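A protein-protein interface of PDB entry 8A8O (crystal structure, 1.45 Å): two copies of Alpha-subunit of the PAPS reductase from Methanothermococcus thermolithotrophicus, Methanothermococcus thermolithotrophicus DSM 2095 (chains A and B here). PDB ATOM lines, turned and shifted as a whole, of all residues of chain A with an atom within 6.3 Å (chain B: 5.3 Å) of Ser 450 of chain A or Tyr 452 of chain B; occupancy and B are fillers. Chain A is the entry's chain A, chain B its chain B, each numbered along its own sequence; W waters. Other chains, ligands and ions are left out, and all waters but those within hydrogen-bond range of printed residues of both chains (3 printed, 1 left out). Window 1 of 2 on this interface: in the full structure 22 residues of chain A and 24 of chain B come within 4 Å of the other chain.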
ATOM      1  N   LEU A 285     -19.084 -19.953 -28.135  1.00  0.00           N
ATOM      2  CA  LEU A 285     -18.813 -21.108 -27.285  1.00  0.00           C
ATOM      3  C   LEU A 285     -17.342 -21.490 -27.327  1.00  0.00           C
ATOM      4  O   LEU A 285     -16.776 -21.929 -26.317  1.00  0.00           O
ATOM      5  CB  LEU A 285     -19.674 -22.280 -27.742  1.00  0.00           C
ATOM      6  CG  LEU A 285     -21.118 -22.268 -27.256  1.00  0.00           C
ATOM      7  CD1 LEU A 285     -21.881 -23.419 -27.889  1.00  0.00           C
ATOM      8  CD2 LEU A 285     -21.176 -22.358 -25.745  1.00  0.00           C
ATOM      9  N   ASP A 443     -36.888 -22.259 -19.999  1.00  0.00           N
ATOM     10  CA  ASP A 443     -35.489 -21.941 -20.273  1.00  0.00           C
ATOM     11  C   ASP A 443     -34.583 -23.112 -19.904  1.00  0.00           C
ATOM     12  O   ASP A 443     -33.698 -23.494 -20.679  1.00  0.00           O
ATOM     13  CB  ASP A 443     -35.093 -20.680 -19.508  1.00  0.00           C
ATOM     14  CG  ASP A 443     -33.605 -20.370 -19.588  1.00  0.00           C
ATOM     15  OD1 ASP A 443     -33.151 -19.738 -20.579  1.00  0.00           O
ATOM     16  OD2 ASP A 443     -32.888 -20.740 -18.634  1.00  0.00           O
ATOM     17  N   GLU A 444     -34.813 -23.722 -18.744  1.00  0.00           N
ATOM     18  CA  GLU A 444     -33.910 -24.750 -18.231  1.00  0.00           C
ATOM     19  C   GLU A 444     -34.195 -26.147 -18.764  1.00  0.00           C
ATOM     20  O   GLU A 444     -33.264 -26.953 -18.882  1.00  0.00           O
ATOM     21  CB  GLU A 444     -33.963 -24.759 -16.700  1.00  0.00           C
ATOM     22  CG  GLU A 444     -33.299 -23.518 -16.111  1.00  0.00           C
ATOM     23  CD  GLU A 444     -33.530 -23.328 -14.616  1.00  0.00           C
ATOM     24  OE1 GLU A 444     -34.136 -24.208 -13.969  1.00  0.00           O
ATOM     25  OE2 GLU A 444     -33.121 -22.266 -14.102  1.00  0.00           O
ATOM     26  N   GLY A 447     -34.960 -26.002 -23.663  1.00  0.00           N
ATOM     27  CA  GLY A 447     -34.036 -25.487 -24.653  1.00  0.00           C
ATOM     28  C   GLY A 447     -34.075 -23.989 -24.847  1.00  0.00           C
ATOM     29  O   GLY A 447     -34.141 -23.497 -25.979  1.00  0.00           O
ATOM     30  N   GLY A 448     -34.021 -23.247 -23.746  1.00  0.00           N
ATOM     31  CA  GLY A 448     -33.906 -21.808 -23.796  1.00  0.00           C
ATOM     32  C   GLY A 448     -32.467 -21.344 -23.948  1.00  0.00           C
ATOM     33  O   GLY A 448     -31.551 -22.120 -24.217  1.00  0.00           O
ATOM     34  N   ILE A 449     -32.284 -20.039 -23.747  1.00  0.00           N
ATOM     35  CA  ILE A 449     -30.976 -19.409 -23.892  1.00  0.00           C
ATOM     36  C   ILE A 449     -29.933 -20.092 -23.015  1.00  0.00           C
ATOM     37  O   ILE A 449     -28.776 -20.259 -23.417  1.00  0.00           O
ATOM     38  CB  ILE A 449     -31.091 -17.908 -23.556  1.00  0.00           C
ATOM     39  CG1 ILE A 449     -31.871 -17.176 -24.656  1.00  0.00           C
ATOM     40  CG2 ILE A 449     -29.733 -17.278 -23.407  1.00  0.00           C
ATOM     41  CD1 ILE A 449     -32.367 -15.803 -24.257  1.00  0.00           C
ATOM     42  N   SER A 450     -30.309 -20.468 -21.790  1.00  0.00           N
ATOM     43  CA  SER A 450     -29.306 -20.953 -20.847  1.00  0.00           C
ATOM     44  C   SER A 450     -28.692 -22.289 -21.263  1.00  0.00           C
ATOM     45  O   SER A 450     -27.589 -22.622 -20.806  1.00  0.00           O
ATOM     46  CB  SER A 450     -29.900 -21.060 -19.443  1.00  0.00           C
ATOM     47  OG  SER A 450     -30.799 -22.146 -19.363  1.00  0.00           O
ATOM     48  N   SER A 451     -29.383 -23.076 -22.087  1.00  0.00           N
ATOM     49  CA  SER A 451     -28.822 -24.308 -22.621  1.00  0.00           C
ATOM     50  C   SER A 451     -28.350 -24.145 -24.059  1.00  0.00           C
ATOM     51  O   SER A 451     -28.139 -25.140 -24.761  1.00  0.00           O
ATOM     52  CB  SER A 451     -29.826 -25.450 -22.502  1.00  0.00           C
ATOM     53  OG  SER A 451     -30.846 -25.318 -23.467  1.00  0.00           O
ATOM     54  N   TYR A 452     -28.173 -22.905 -24.512  1.00  0.00           N
ATOM     55  CA  TYR A 452     -27.767 -22.648 -25.890  1.00  0.00           C
ATOM     56  C   TYR A 452     -28.741 -23.301 -26.864  1.00  0.00           C
ATOM     57  O   TYR A 452     -28.353 -23.803 -27.921  1.00  0.00           O
ATOM     58  CB  TYR A 452     -26.343 -23.124 -26.154  1.00  0.00           C
ATOM     59  CG  TYR A 452     -25.352 -22.588 -25.162  1.00  0.00           C
ATOM     60  CD1 TYR A 452     -25.105 -21.225 -25.075  1.00  0.00           C
ATOM     61  CD2 TYR A 452     -24.675 -23.439 -24.294  1.00  0.00           C
ATOM     62  CE1 TYR A 452     -24.203 -20.722 -24.162  1.00  0.00           C
ATOM     63  CE2 TYR A 452     -23.769 -22.946 -23.377  1.00  0.00           C
ATOM     64  CZ  TYR A 452     -23.537 -21.587 -23.315  1.00  0.00           C
ATOM     65  OH  TYR A 452     -22.635 -21.097 -22.402  1.00  0.00           O
ATOM     66  N   TYR A 453     -30.016 -23.314 -26.480  1.00  0.00           N
ATOM     67  CA  TYR A 453     -31.140 -23.777 -27.286  1.00  0.00           C
ATOM     68  C   TYR A 453     -31.208 -25.289 -27.443  1.00  0.00           C
ATOM     69  O   TYR A 453     -32.063 -25.776 -28.192  1.00  0.00           O
ATOM     70  CB  TYR A 453     -31.160 -23.098 -28.657  1.00  0.00           C
ATOM     71  CG  TYR A 453     -30.967 -21.602 -28.593  1.00  0.00           C
ATOM     72  CD1 TYR A 453     -31.893 -20.784 -27.936  1.00  0.00           C
ATOM     73  CD2 TYR A 453     -29.888 -20.997 -29.218  1.00  0.00           C
ATOM     74  CE1 TYR A 453     -31.728 -19.406 -27.898  1.00  0.00           C
ATOM     75  CE2 TYR A 453     -29.717 -19.624 -29.184  1.00  0.00           C
ATOM     76  CZ  TYR A 453     -30.638 -18.836 -28.527  1.00  0.00           C
ATOM     77  OH  TYR A 453     -30.449 -17.478 -28.518  1.00  0.00           O
ATOM     78  N   LYS A 459     -34.800 -33.812 -20.159  1.00  0.00           N
ATOM     79  CA  LYS A 459     -35.204 -32.487 -19.714  1.00  0.00           C
ATOM     80  C   LYS A 459     -36.635 -32.177 -20.132  1.00  0.00           C
ATOM     81  O   LYS A 459     -37.394 -31.579 -19.355  1.00  0.00           O
ATOM     82  CB  LYS A 459     -34.219 -31.436 -20.227  1.00  0.00           C
ATOM     83  CG  LYS A 459     -32.850 -31.601 -19.597  1.00  0.00           C
ATOM     84  CD  LYS A 459     -31.910 -30.450 -19.843  1.00  0.00           C
ATOM     85  CE  LYS A 459     -30.845 -30.395 -18.744  1.00  0.00           C
ATOM     86  NZ  LYS A 459     -29.651 -29.575 -19.108  1.00  0.00           N
ATOM     87  N   LEU B 281     -20.672 -30.751 -15.797  1.00  0.00           N
ATOM     88  CA  LEU B 281     -20.865 -29.779 -16.868  1.00  0.00           C
ATOM     89  C   LEU B 281     -20.823 -30.459 -18.229  1.00  0.00           C
ATOM     90  O   LEU B 281     -21.660 -30.176 -19.095  1.00  0.00           O
ATOM     91  CB  LEU B 281     -19.791 -28.699 -16.777  1.00  0.00           C
ATOM     92  CG  LEU B 281     -19.921 -27.674 -15.652  1.00  0.00           C
ATOM     93  CD1 LEU B 281     -19.006 -26.489 -15.961  1.00  0.00           C
ATOM     94  CD2 LEU B 281     -21.346 -27.189 -15.446  1.00  0.00           C
ATOM     95  N   ASN B 284     -24.121 -32.332 -18.978  1.00  0.00           N
ATOM     96  CA  ASN B 284     -25.184 -31.410 -19.366  1.00  0.00           C
ATOM     97  C   ASN B 284     -24.929 -30.825 -20.749  1.00  0.00           C
ATOM     98  O   ASN B 284     -25.831 -30.784 -21.595  1.00  0.00           O
ATOM     99  CB  ASN B 284     -25.314 -30.291 -18.334  1.00  0.00           C
ATOM    100  CG  ASN B 284     -26.164 -30.696 -17.142  1.00  0.00           C
ATOM    101  OD1 ASN B 284     -27.393 -30.707 -17.212  1.00  0.00           O
ATOM    102  ND2 ASN B 284     -25.514 -31.001 -16.036  1.00  0.00           N
ATOM    103  N   LEU B 285     -23.700 -30.373 -21.000  1.00  0.00           N
ATOM    104  CA  LEU B 285     -23.400 -29.753 -22.287  1.00  0.00           C
ATOM    105  C   LEU B 285     -23.601 -30.733 -23.429  1.00  0.00           C
ATOM    106  O   LEU B 285     -24.067 -30.351 -24.509  1.00  0.00           O
ATOM    107  CB  LEU B 285     -21.970 -29.230 -22.294  1.00  0.00           C
ATOM    108  CG  LEU B 285     -21.718 -27.916 -21.562  1.00  0.00           C
ATOM    109  CD1 LEU B 285     -20.285 -27.476 -21.817  1.00  0.00           C
ATOM    110  CD2 LEU B 285     -22.689 -26.836 -22.009  1.00  0.00           C
ATOM    111  N   GLY B 448     -19.127 -16.067 -16.354  1.00  0.00           N
ATOM    112  CA  GLY B 448     -20.164 -16.470 -15.440  1.00  0.00           C
ATOM    113  C   GLY B 448     -20.913 -17.708 -15.906  1.00  0.00           C
ATOM    114  O   GLY B 448     -20.526 -18.423 -16.838  1.00  0.00           O
ATOM    115  N   ILE B 449     -22.011 -17.972 -15.204  1.00  0.00           N
ATOM    116  CA  ILE B 449     -22.860 -19.110 -15.516  1.00  0.00           C
ATOM    117  C   ILE B 449     -23.234 -19.110 -16.990  1.00  0.00           C
ATOM    118  O   ILE B 449     -23.228 -20.156 -17.646  1.00  0.00           O
ATOM    119  CB  ILE B 449     -24.107 -19.100 -14.609  1.00  0.00           C
ATOM    120  CG1 ILE B 449     -23.724 -19.422 -13.165  1.00  0.00           C
ATOM    121  CG2 ILE B 449     -25.139 -20.082 -15.109  1.00  0.00           C
ATOM    122  CD1 ILE B 449     -24.743 -18.979 -12.128  1.00  0.00           C
ATOM    123  N   SER B 450     -23.581 -17.942 -17.531  1.00  0.00           N
ATOM    124  CA  SER B 450     -24.148 -17.915 -18.875  1.00  0.00           C
ATOM    125  C   SER B 450     -23.137 -18.337 -19.935  1.00  0.00           C
ATOM    126  O   SER B 450     -23.540 -18.761 -21.020  1.00  0.00           O
ATOM    127  CB  SER B 450     -24.742 -16.540 -19.171  1.00  0.00           C
ATOM    128  OG  SER B 450     -23.741 -15.618 -19.506  1.00  0.00           O
ATOM    129  N   SER B 451     -21.841 -18.262 -19.641  1.00  0.00           N
ATOM    130  CA  SER B 451     -20.807 -18.722 -20.557  1.00  0.00           C
ATOM    131  C   SER B 451     -20.250 -20.083 -20.155  1.00  0.00           C
ATOM    132  O   SER B 451     -19.189 -20.488 -20.647  1.00  0.00           O
ATOM    133  CB  SER B 451     -19.700 -17.674 -20.678  1.00  0.00           C
ATOM    134  OG  SER B 451     -18.936 -17.590 -19.492  1.00  0.00           O
ATOM    135  N   TYR B 452     -20.959 -20.807 -19.288  1.00  0.00           N
ATOM    136  CA  TYR B 452     -20.473 -22.068 -18.735  1.00  0.00           C
ATOM    137  C   TYR B 452     -19.071 -21.887 -18.159  1.00  0.00           C
ATOM    138  O   TYR B 452     -18.212 -22.763 -18.251  1.00  0.00           O
ATOM    139  CB  TYR B 452     -20.530 -23.187 -19.763  1.00  0.00           C
ATOM    140  CG  TYR B 452     -21.794 -24.000 -19.622  1.00  0.00           C
ATOM    141  CD1 TYR B 452     -23.014 -23.505 -20.069  1.00  0.00           C
ATOM    142  CD2 TYR B 452     -21.774 -25.247 -19.010  1.00  0.00           C
ATOM    143  CE1 TYR B 452     -24.176 -24.245 -19.933  1.00  0.00           C
ATOM    144  CE2 TYR B 452     -22.927 -25.993 -18.866  1.00  0.00           C
ATOM    145  CZ  TYR B 452     -24.126 -25.488 -19.329  1.00  0.00           C
ATOM    146  OH  TYR B 452     -25.276 -26.232 -19.186  1.00  0.00           O
ATOM    147  N   TYR B 453     -18.848 -20.709 -17.578  1.00  0.00           N
ATOM    148  CA  TYR B 453     -17.644 -20.325 -16.849  1.00  0.00           C
ATOM    149  C   TYR B 453     -16.430 -20.076 -17.735  1.00  0.00           C
ATOM    150  O   TYR B 453     -15.334 -19.841 -17.199  1.00  0.00           O
ATOM    151  CB  TYR B 453     -17.281 -21.336 -15.757  1.00  0.00           C
ATOM    152  CG  TYR B 453     -18.444 -21.778 -14.910  1.00  0.00           C
ATOM    153  CD1 TYR B 453     -19.117 -20.867 -14.101  1.00  0.00           C
ATOM    154  CD2 TYR B 453     -18.856 -23.089 -14.893  1.00  0.00           C
ATOM    155  CE1 TYR B 453     -20.181 -21.271 -13.305  1.00  0.00           C
ATOM    156  CE2 TYR B 453     -19.916 -23.499 -14.099  1.00  0.00           C
ATOM    157  CZ  TYR B 453     -20.568 -22.588 -13.307  1.00  0.00           C
ATOM    158  OH  TYR B 453     -21.628 -23.026 -12.537  1.00  0.00           O
ATOM    159  N   ARG B 454     -16.588 -20.088 -19.061  1.00  0.00           N
ATOM    160  CA  ARG B 454     -15.460 -19.921 -19.967  1.00  0.00           C
ATOM    161  C   ARG B 454     -15.127 -18.451 -20.159  1.00  0.00           C
ATOM    162  O   ARG B 454     -16.018 -17.602 -20.262  1.00  0.00           O
ATOM    163  CB  ARG B 454     -15.772 -20.540 -21.334  1.00  0.00           C
ATOM    164  CG  ARG B 454     -16.149 -22.010 -21.287  1.00  0.00           C
ATOM    165  CD  ARG B 454     -16.819 -22.443 -22.575  1.00  0.00           C
ATOM    166  NE  ARG B 454     -17.263 -23.829 -22.508  1.00  0.00           N
ATOM    167  CZ  ARG B 454     -17.721 -24.521 -23.542  1.00  0.00           C
ATOM    168  NH1 ARG B 454     -17.795 -23.989 -24.750  1.00  0.00           N
ATOM    169  NH2 ARG B 454     -18.120 -25.776 -23.357  1.00  0.00           N
HETATM  170  O   HOH W   1     -26.630 -18.894 -21.851  1.00  0.00           O
HETATM  171  O   HOH W   2     -28.187 -32.050 -21.012  1.00  0.00           O
HETATM  172  O   HOH W   3     -25.974 -20.976 -18.827  1.00  0.00           O
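Water W2 lies within hydrogen-bond range of O of Asn 284 of chain B (2.7 Å) and NZ of Lys 459 of chain A (3.4 Å). Water W1 bridges the backbone carbonyl oxygen of Ile 449 of chain A (3.0 Å) and the backbone carbonyl oxygen of Ser 450 of chain B (3.2 Å). Water W3 bridges the backbone carbonyl oxygen (O) of Ser 450 of chain A (3.0 Å) and the backbone carbonyl oxygen (O) of Ile 449 of chain B (3.1 Å).
Of the 11 printed residues of chain A, 4 touch a printed residue of chain B. Hydrophobic or aromatic side chains of chain A that line the printed part of chain B: Leu 285 and Tyr 452. Among the printed residues, 6 pairs touch across the chains.
The side-chain hydroxyl (OG) of Ser 450 of chain A sits at hydrogen-bond distance from the side-chain carboxylate (OD2) of Asp 443 of chain A, at 2.6 Å. O of Gly 448 of chain B sits at hydrogen-bond distance from OG of Ser 451 of chain B, at 3.2 Å. OG of Ser 451 of chain B is in hydrogen-bond range of O of Arg 454 of chain B.
Ser 450 of chain A touches Tyr 452 of chain B, and with the chains exchanged Tyr 452 of chain A touches Ser 450 of chain B. Tyr 452 of chain A touches Ser 451 of chain B, but with the chains exchanged Ser 451 of chain A does not touch Tyr 452 of chain B (5.3 Å). Tyr 452 of chain A touches its own counterpart, Tyr 452 of chain B. Positions printed for both chains: 285, 448, 449, 450, 451, 452 and 453. Of the 6 pairs that touch across the chains among the printed residues, 3 have their exchanged pair printed and touching as well.
The side-chain amide oxygen (OD1) of Asn 284 of chain B is in hydrogen-bond range of the side-chain amino group (NZ) of Lys 459 of chain A (3.2 Å). The side-chain hydroxyl (OH) of Tyr 452 of chain A sits at hydrogen-bond distance from the backbone carbonyl oxygen (O) of Ser 450 of chain B. The guanidinium group (NH1) of Arg 454 of chain B sits at hydrogen-bond distance from the backbone carbonyl oxygen (O) of Leu 285 of chain A, at 2.8 Å.
Among the printed residues, pairs that only touch across the chains: Tyr 452 of chain A with Tyr 452 of chain B (3.4 Å), Tyr 452 of chain A with Ser 451 of chain B (3.4 Å) and Ser 450 of chain A with Tyr 452 of chain B (3.9 Å).
Printed residues of chain B within 4 Å of Leu 285 of chain A: Arg 454. Gly 448 of chain A touches none of the printed residues of chain B. Ser 450 of chain A touches just one residue of chain B: Tyr 452. Of the printed residues of chain B, Lys 459 of chain A touches Asn 284. Leu 281 of chain B touches none of the printed residues of chain A. Printed residues of chain A within 4 Å of Ser 451 of chain B: Tyr 452 (3.4 Å). Tyr 452 of chain B touches two residues of chain A. The nearest printed residue of chain A that does not touch Asn 284 of chain B is Ser 451 of chain A (6.7 Å).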
